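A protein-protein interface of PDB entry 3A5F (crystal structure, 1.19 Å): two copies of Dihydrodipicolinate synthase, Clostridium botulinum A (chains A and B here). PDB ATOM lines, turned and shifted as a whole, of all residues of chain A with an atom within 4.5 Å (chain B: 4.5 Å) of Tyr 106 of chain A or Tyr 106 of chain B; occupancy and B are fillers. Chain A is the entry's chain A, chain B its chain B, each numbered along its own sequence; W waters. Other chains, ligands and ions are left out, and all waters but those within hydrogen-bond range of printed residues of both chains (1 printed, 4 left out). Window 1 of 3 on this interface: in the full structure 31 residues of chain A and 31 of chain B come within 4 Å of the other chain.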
ATOM      1  N   SER A  79       5.006 -28.188 -19.590  1.00  0.00           N
ATOM      2  CA  SER A  79       4.145 -27.361 -18.751  1.00  0.00           C
ATOM      3  C   SER A  79       5.036 -26.434 -17.960  1.00  0.00           C
ATOM      4  O   SER A  79       6.216 -26.256 -18.265  1.00  0.00           O
ATOM      5  CB  SER A  79       3.282 -28.219 -17.811  1.00  0.00           C
ATOM      6  OG  SER A  79       4.141 -28.881 -16.878  1.00  0.00           O
ATOM      7  N   ASN A  80       4.418 -25.754 -17.009  1.00  0.00           N
ATOM      8  CA  ASN A  80       5.123 -24.806 -16.174  1.00  0.00           C
ATOM      9  C   ASN A  80       5.823 -25.403 -14.963  1.00  0.00           C
ATOM     10  O   ASN A  80       6.454 -24.698 -14.188  1.00  0.00           O
ATOM     11  CB  ASN A  80       4.238 -23.639 -15.817  1.00  0.00           C
ATOM     12  CG  ASN A  80       3.001 -23.990 -15.092  1.00  0.00           C
ATOM     13  OD1 ASN A  80       2.722 -25.201 -14.928  1.00  0.00           O
ATOM     14  ND2 ASN A  80       2.248 -22.998 -14.676  1.00  0.00           N
ATOM     15  N   ILE A 103       6.646 -25.862 -24.326  1.00  0.00           N
ATOM     16  CA  ILE A 103       6.393 -24.475 -24.041  1.00  0.00           C
ATOM     17  C   ILE A 103       7.365 -23.977 -22.976  1.00  0.00           C
ATOM     18  O   ILE A 103       7.812 -24.686 -22.086  1.00  0.00           O
ATOM     19  CB  ILE A 103       4.928 -24.278 -23.659  1.00  0.00           C
ATOM     20  CG1 ILE A 103       4.537 -22.783 -23.808  1.00  0.00           C
ATOM     21  CG2 ILE A 103       4.611 -24.924 -22.316  1.00  0.00           C
ATOM     22  CD1 ILE A 103       3.024 -22.579 -23.770  1.00  0.00           C
ATOM     23  N   THR A 104       7.637 -22.674 -23.022  1.00  0.00           N
ATOM     24  CA  THR A 104       8.244 -22.019 -21.850  1.00  0.00           C
ATOM     25  C   THR A 104       7.321 -22.187 -20.648  1.00  0.00           C
ATOM     26  O   THR A 104       6.087 -22.302 -20.788  1.00  0.00           O
ATOM     27  CB  THR A 104       8.522 -20.555 -22.083  1.00  0.00           C
ATOM     28  OG1 THR A 104       7.279 -19.873 -22.167  1.00  0.00           O
ATOM     29  CG2 THR A 104       9.292 -20.280 -23.324  1.00  0.00           C
ATOM     30  N   PRO A 105       7.838 -22.032 -19.434  1.00  0.00           N
ATOM     31  CA  PRO A 105       6.939 -21.837 -18.297  1.00  0.00           C
ATOM     32  C   PRO A 105       6.069 -20.611 -18.524  1.00  0.00           C
ATOM     33  O   PRO A 105       6.302 -19.730 -19.427  1.00  0.00           O
ATOM     34  CB  PRO A 105       7.908 -21.616 -17.183  1.00  0.00           C
ATOM     35  CG  PRO A 105       9.157 -22.374 -17.570  1.00  0.00           C
ATOM     36  CD  PRO A 105       9.227 -22.222 -19.071  1.00  0.00           C
ATOM     37  N   TYR A 106       4.957 -20.621 -17.864  1.00  0.00           N
ATOM     38  CA  TYR A 106       3.872 -19.689 -17.986  1.00  0.00           C
ATOM     39  C   TYR A 106       3.286 -19.560 -16.620  1.00  0.00           C
ATOM     40  O   TYR A 106       3.239 -20.495 -15.839  1.00  0.00           O
ATOM     41  CB  TYR A 106       2.803 -20.174 -18.963  1.00  0.00           C
ATOM     42  CG  TYR A 106       2.340 -21.598 -18.799  1.00  0.00           C
ATOM     43  CD1 TYR A 106       1.317 -21.912 -17.939  1.00  0.00           C
ATOM     44  CD2 TYR A 106       2.905 -22.639 -19.514  1.00  0.00           C
ATOM     45  CE1 TYR A 106       0.865 -23.186 -17.838  1.00  0.00           C
ATOM     46  CE2 TYR A 106       2.493 -23.894 -19.383  1.00  0.00           C
ATOM     47  CZ  TYR A 106       1.452 -24.212 -18.555  1.00  0.00           C
ATOM     48  OH  TYR A 106       1.051 -25.504 -18.412  1.00  0.00           O
ATOM     49  N   TYR A 107       2.800 -18.335 -16.330  1.00  0.00           N
ATOM     50  CA  TYR A 107       2.153 -17.974 -15.060  1.00  0.00           C
ATOM     51  C   TYR A 107       3.181 -17.895 -13.931  1.00  0.00           C
ATOM     52  O   TYR A 107       3.459 -16.778 -13.465  1.00  0.00           O
ATOM     53  CB  TYR A 107       0.909 -18.832 -14.795  1.00  0.00           C
ATOM     54  CG  TYR A 107       0.432 -18.713 -13.355  1.00  0.00           C
ATOM     55  CD1 TYR A 107       0.233 -17.488 -12.752  1.00  0.00           C
ATOM     56  CD2 TYR A 107       0.276 -19.824 -12.605  1.00  0.00           C
ATOM     57  CE1 TYR A 107      -0.058 -17.400 -11.419  1.00  0.00           C
ATOM     58  CE2 TYR A 107      -0.031 -19.785 -11.298  1.00  0.00           C
ATOM     59  CZ  TYR A 107      -0.197 -18.533 -10.690  1.00  0.00           C
ATOM     60  OH  TYR A 107      -0.479 -18.509  -9.344  1.00  0.00           O
ATOM     61  N   ASN A 108       3.746 -18.999 -13.508  1.00  0.00           N
ATOM     62  CA  ASN A 108       4.869 -18.903 -12.594  1.00  0.00           C
ATOM     63  C   ASN A 108       6.047 -18.221 -13.222  1.00  0.00           C
ATOM     64  O   ASN A 108       6.722 -17.433 -12.545  1.00  0.00           O
ATOM     65  CB  ASN A 108       5.226 -20.261 -11.954  1.00  0.00           C
ATOM     66  CG  ASN A 108       5.718 -21.334 -12.908  1.00  0.00           C
ATOM     67  OD1 ASN A 108       5.521 -21.214 -14.135  1.00  0.00           O
ATOM     68  ND2 ASN A 108       6.343 -22.372 -12.360  1.00  0.00           N
ATOM     69  N   LYS A 109       6.281 -18.486 -14.490  1.00  0.00           N
ATOM     70  CA  LYS A 109       7.392 -17.917 -15.203  1.00  0.00           C
ATOM     71  C   LYS A 109       8.696 -18.338 -14.579  1.00  0.00           C
ATOM     72  O   LYS A 109       8.771 -19.274 -13.763  1.00  0.00           O
ATOM     73  CB  LYS A 109       7.234 -16.385 -15.384  1.00  0.00           C
ATOM     74  CG  LYS A 109       5.935 -16.047 -16.078  1.00  0.00           C
ATOM     75  CD  LYS A 109       5.686 -14.489 -16.214  1.00  0.00           C
ATOM     76  CE  LYS A 109       6.677 -13.586 -16.396  1.00  0.00           C
ATOM     77  NZ  LYS A 109       6.150 -12.208 -16.486  1.00  0.00           N
ATOM     78  N   THR A 139       1.902 -16.702 -22.122  1.00  0.00           N
ATOM     79  CA  THR A 139       2.683 -17.210 -20.983  1.00  0.00           C
ATOM     80  C   THR A 139       3.152 -16.124 -20.019  1.00  0.00           C
ATOM     81  O   THR A 139       3.540 -16.409 -18.911  1.00  0.00           O
ATOM     82  CB  THR A 139       3.919 -17.944 -21.481  1.00  0.00           C
ATOM     83  OG1 THR A 139       4.714 -16.941 -22.136  1.00  0.00           O
ATOM     84  CG2 THR A 139       3.633 -19.112 -22.408  1.00  0.00           C
ATOM     85  N   SER B  79      -7.094 -22.761 -11.100  1.00  0.00           N
ATOM     86  CA  SER B  79      -6.217 -23.113 -12.189  1.00  0.00           C
ATOM     87  C   SER B  79      -6.799 -22.639 -13.503  1.00  0.00           C
ATOM     88  O   SER B  79      -7.839 -21.967 -13.522  1.00  0.00           O
ATOM     89  CB  SER B  79      -5.811 -24.548 -12.200  1.00  0.00           C
ATOM     90  OG  SER B  79      -6.766 -25.297 -12.649  1.00  0.00           O
ATOM     91  N   ASN B  80      -6.171 -22.980 -14.584  1.00  0.00           N
ATOM     92  CA  ASN B  80      -6.649 -22.671 -15.892  1.00  0.00           C
ATOM     93  C   ASN B  80      -7.587 -23.696 -16.470  1.00  0.00           C
ATOM     94  O   ASN B  80      -8.074 -23.543 -17.583  1.00  0.00           O
ATOM     95  CB  ASN B  80      -5.462 -22.332 -16.813  1.00  0.00           C
ATOM     96  CG  ASN B  80      -4.498 -23.446 -16.952  1.00  0.00           C
ATOM     97  OD1 ASN B  80      -4.619 -24.465 -16.291  1.00  0.00           O
ATOM     98  ND2 ASN B  80      -3.537 -23.284 -17.874  1.00  0.00           N
ATOM     99  N   ILE B 103      -7.468 -17.534  -9.359  1.00  0.00           N
ATOM    100  CA  ILE B 103      -6.862 -16.835 -10.471  1.00  0.00           C
ATOM    101  C   ILE B 103      -7.741 -16.931 -11.701  1.00  0.00           C
ATOM    102  O   ILE B 103      -8.463 -17.863 -11.952  1.00  0.00           O
ATOM    103  CB  ILE B 103      -5.457 -17.380 -10.698  1.00  0.00           C
ATOM    104  CG1 ILE B 103      -4.598 -16.415 -11.564  1.00  0.00           C
ATOM    105  CG2 ILE B 103      -5.502 -18.799 -11.229  1.00  0.00           C
ATOM    106  CD1 ILE B 103      -3.122 -16.707 -11.560  1.00  0.00           C
ATOM    107  N   THR B 104      -7.588 -15.929 -12.550  1.00  0.00           N
ATOM    108  CA  THR B 104      -8.107 -16.057 -13.916  1.00  0.00           C
ATOM    109  C   THR B 104      -7.412 -17.262 -14.596  1.00  0.00           C
ATOM    110  O   THR B 104      -6.280 -17.597 -14.269  1.00  0.00           O
ATOM    111  CB  THR B 104      -7.927 -14.847 -14.739  1.00  0.00           C
ATOM    112  OG1 THR B 104      -6.539 -14.656 -14.994  1.00  0.00           O
ATOM    113  CG2 THR B 104      -8.461 -13.589 -14.104  1.00  0.00           C
ATOM    114  N   PRO B 105      -8.040 -17.801 -15.628  1.00  0.00           N
ATOM    115  CA  PRO B 105      -7.264 -18.673 -16.529  1.00  0.00           C
ATOM    116  C   PRO B 105      -6.076 -17.963 -17.067  1.00  0.00           C
ATOM    117  O   PRO B 105      -5.914 -16.696 -17.033  1.00  0.00           O
ATOM    118  CB  PRO B 105      -8.267 -18.957 -17.603  1.00  0.00           C
ATOM    119  CG  PRO B 105      -9.607 -18.888 -16.988  1.00  0.00           C
ATOM    120  CD  PRO B 105      -9.453 -17.765 -15.947  1.00  0.00           C
ATOM    121  N   TYR B 106      -5.069 -18.750 -17.376  1.00  0.00           N
ATOM    122  CA  TYR B 106      -3.754 -18.327 -17.783  1.00  0.00           C
ATOM    123  C   TYR B 106      -3.307 -19.289 -18.849  1.00  0.00           C
ATOM    124  O   TYR B 106      -3.633 -20.467 -18.813  1.00  0.00           O
ATOM    125  CB  TYR B 106      -2.753 -18.311 -16.644  1.00  0.00           C
ATOM    126  CG  TYR B 106      -2.759 -19.500 -15.766  1.00  0.00           C
ATOM    127  CD1 TYR B 106      -1.962 -20.621 -16.065  1.00  0.00           C
ATOM    128  CD2 TYR B 106      -3.519 -19.569 -14.626  1.00  0.00           C
ATOM    129  CE1 TYR B 106      -1.946 -21.700 -15.263  1.00  0.00           C
ATOM    130  CE2 TYR B 106      -3.495 -20.690 -13.826  1.00  0.00           C
ATOM    131  CZ  TYR B 106      -2.735 -21.784 -14.136  1.00  0.00           C
ATOM    132  OH  TYR B 106      -2.722 -22.868 -13.338  1.00  0.00           O
ATOM    133  N   TYR B 107      -2.530 -18.764 -19.804  1.00  0.00           N
ATOM    134  CA  TYR B 107      -1.941 -19.580 -20.901  1.00  0.00           C
ATOM    135  C   TYR B 107      -3.029 -19.964 -21.907  1.00  0.00           C
ATOM    136  O   TYR B 107      -3.005 -19.447 -23.024  1.00  0.00           O
ATOM    137  CB  TYR B 107      -1.055 -20.697 -20.412  1.00  0.00           C
ATOM    138  CG  TYR B 107      -0.747 -21.715 -21.486  1.00  0.00           C
ATOM    139  CD1 TYR B 107      -0.286 -21.341 -22.700  1.00  0.00           C
ATOM    140  CD2 TYR B 107      -0.986 -23.032 -21.272  1.00  0.00           C
ATOM    141  CE1 TYR B 107      -0.144 -22.239 -23.740  1.00  0.00           C
ATOM    142  CE2 TYR B 107      -0.814 -23.962 -22.239  1.00  0.00           C
ATOM    143  CZ  TYR B 107      -0.415 -23.578 -23.478  1.00  0.00           C
ATOM    144  OH  TYR B 107      -0.235 -24.505 -24.517  1.00  0.00           O
ATOM    145  N   ASN B 108      -3.953 -20.845 -21.553  1.00  0.00           N
ATOM    146  CA  ASN B 108      -5.086 -21.099 -22.439  1.00  0.00           C
ATOM    147  C   ASN B 108      -5.959 -19.830 -22.560  1.00  0.00           C
ATOM    148  O   ASN B 108      -6.408 -19.541 -23.646  1.00  0.00           O
ATOM    149  CB  ASN B 108      -5.902 -22.314 -22.052  1.00  0.00           C
ATOM    150  CG  ASN B 108      -6.578 -22.226 -20.678  1.00  0.00           C
ATOM    151  OD1 ASN B 108      -6.187 -21.411 -19.828  1.00  0.00           O
ATOM    152  ND2 ASN B 108      -7.492 -23.177 -20.454  1.00  0.00           N
ATOM    153  N   LYS B 109      -6.084 -19.080 -21.481  1.00  0.00           N
ATOM    154  CA  LYS B 109      -6.878 -17.906 -21.443  1.00  0.00           C
ATOM    155  C   LYS B 109      -8.324 -18.198 -21.782  1.00  0.00           C
ATOM    156  O   LYS B 109      -8.740 -19.367 -21.772  1.00  0.00           O
ATOM    157  CB  LYS B 109      -6.271 -16.788 -22.302  1.00  0.00           C
ATOM    158  CG  LYS B 109      -4.810 -16.450 -21.873  1.00  0.00           C
ATOM    159  CD  LYS B 109      -4.155 -15.339 -22.794  1.00  0.00           C
ATOM    160  CE  LYS B 109      -4.951 -14.214 -23.346  1.00  0.00           C
ATOM    161  NZ  LYS B 109      -3.930 -13.478 -24.165  1.00  0.00           N
ATOM    162  N   THR B 139      -0.518 -14.058 -16.520  1.00  0.00           N
ATOM    163  CA  THR B 139      -1.527 -14.923 -17.119  1.00  0.00           C
ATOM    164  C   THR B 139      -1.752 -14.690 -18.583  1.00  0.00           C
ATOM    165  O   THR B 139      -2.346 -15.534 -19.266  1.00  0.00           O
ATOM    166  CB  THR B 139      -2.868 -14.760 -16.403  1.00  0.00           C
ATOM    167  OG1 THR B 139      -3.276 -13.417 -16.670  1.00  0.00           O
ATOM    168  CG2 THR B 139      -2.789 -15.031 -14.906  1.00  0.00           C
HETATM  169  O   HOH W   1       0.279 -17.697 -18.408  1.00  0.00           O
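Hydrophobic or aromatic side chains of chain A within 4 Å of the printed part of chain B: Ile 103, Tyr 106 and Tyr 107.
Of the 10 printed residues of chain B, 3 touch a printed residue of chain A.
Hydrophobic or aromatic side chains of chain B within 4 Å of the printed part of chain A: Ile 103, Tyr 106 and Tyr 107.
Among the printed residues, no Asp or Glu carboxylate lies within 4 Å of a Lys or Arg side-chain nitrogen of the other chain.
Water W1 lies within hydrogen-bond range of the backbone NH of Tyr 107 of chain B (3.3 Å) and the backbone NH of Tyr 107 of chain A (3.3 Å).
Of the printed residues of chain B, Ile 103 of chain A touches Tyr 107 (3.2 Å).
Pro 105 of chain A touches none of the printed residues of chain B.
Printed residues of chain B within 4 Å of Tyr 106 of chain A: Tyr 106 and Tyr 107.
Of the printed residues of chain B, Tyr 107 of chain A touches Ile 103 and Tyr 106.
Of the printed residues of chain A, Tyr 106 of chain B touches Tyr 106 and Tyr 107.
Printed residues of chain A within 4 Å of Tyr 107 of chain B: Ile 103 and Tyr 106.
The nearest printed residue of chain A that does not touch Tyr 106 of chain B is Asn 80 of chain A (4.4 Å).
Ile 103 of chain A touches Tyr 107 of chain B, and with the chains exchanged Tyr 107 of chain A touches Ile 103 of chain B.
Tyr 106 of chain A touches its own counterpart, Tyr 106 of chain B.
Tyr 106 of chain A touches Tyr 107 of chain B, and with the chains exchanged Tyr 107 of chain A touches Tyr 106 of chain B.
Positions printed for both chains: 79, 80, 103, 104, 105, 106, 107, 108, 109 and 139.
ND2 of Asn 80 of chain A lies within hydrogen-bond range of O of Tyr 106 of chain A (2.9 Å).
OD1 of Asn 108 of chain A lies close to O of Tyr 106 of chain A (2.9 Å).
N of Tyr 107 of chain A sits at hydrogen-bond distance from O of Thr 139 of chain A, 3.3 Å away.
The side-chain amide nitrogen of Asn 80 of chain B sits at hydrogen-bond distance from the backbone carbonyl oxygen of Tyr 106 of chain B (3.0 Å).
The backbone carbonyl oxygen (O) of Tyr 106 of chain B lies close to the side-chain amide oxygen (OD1) of Asn 108 of chain B, 2.9 Å away.
N of Tyr 107 of chain B lies within hydrogen-bond range of O of Thr 139 of chain B (3.3 Å).
CD1 of Ile 103 of chain A touches CE1 of Tyr 107 of chain B, 3.2 Å away.
CD1 of Tyr 106 of chain A touches CD1 of Tyr 106 of chain B, 3.99 Å away.
Tyr 107 of chain B touches Tyr 106 of chain A.
Tyr 107 of chain A touches Ile 103 of chain B (CE1 to CD1, 3.1 Å).
CB of Tyr 107 of chain A touches CD1 of Tyr 106 of chain B, 3.6 Å away.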
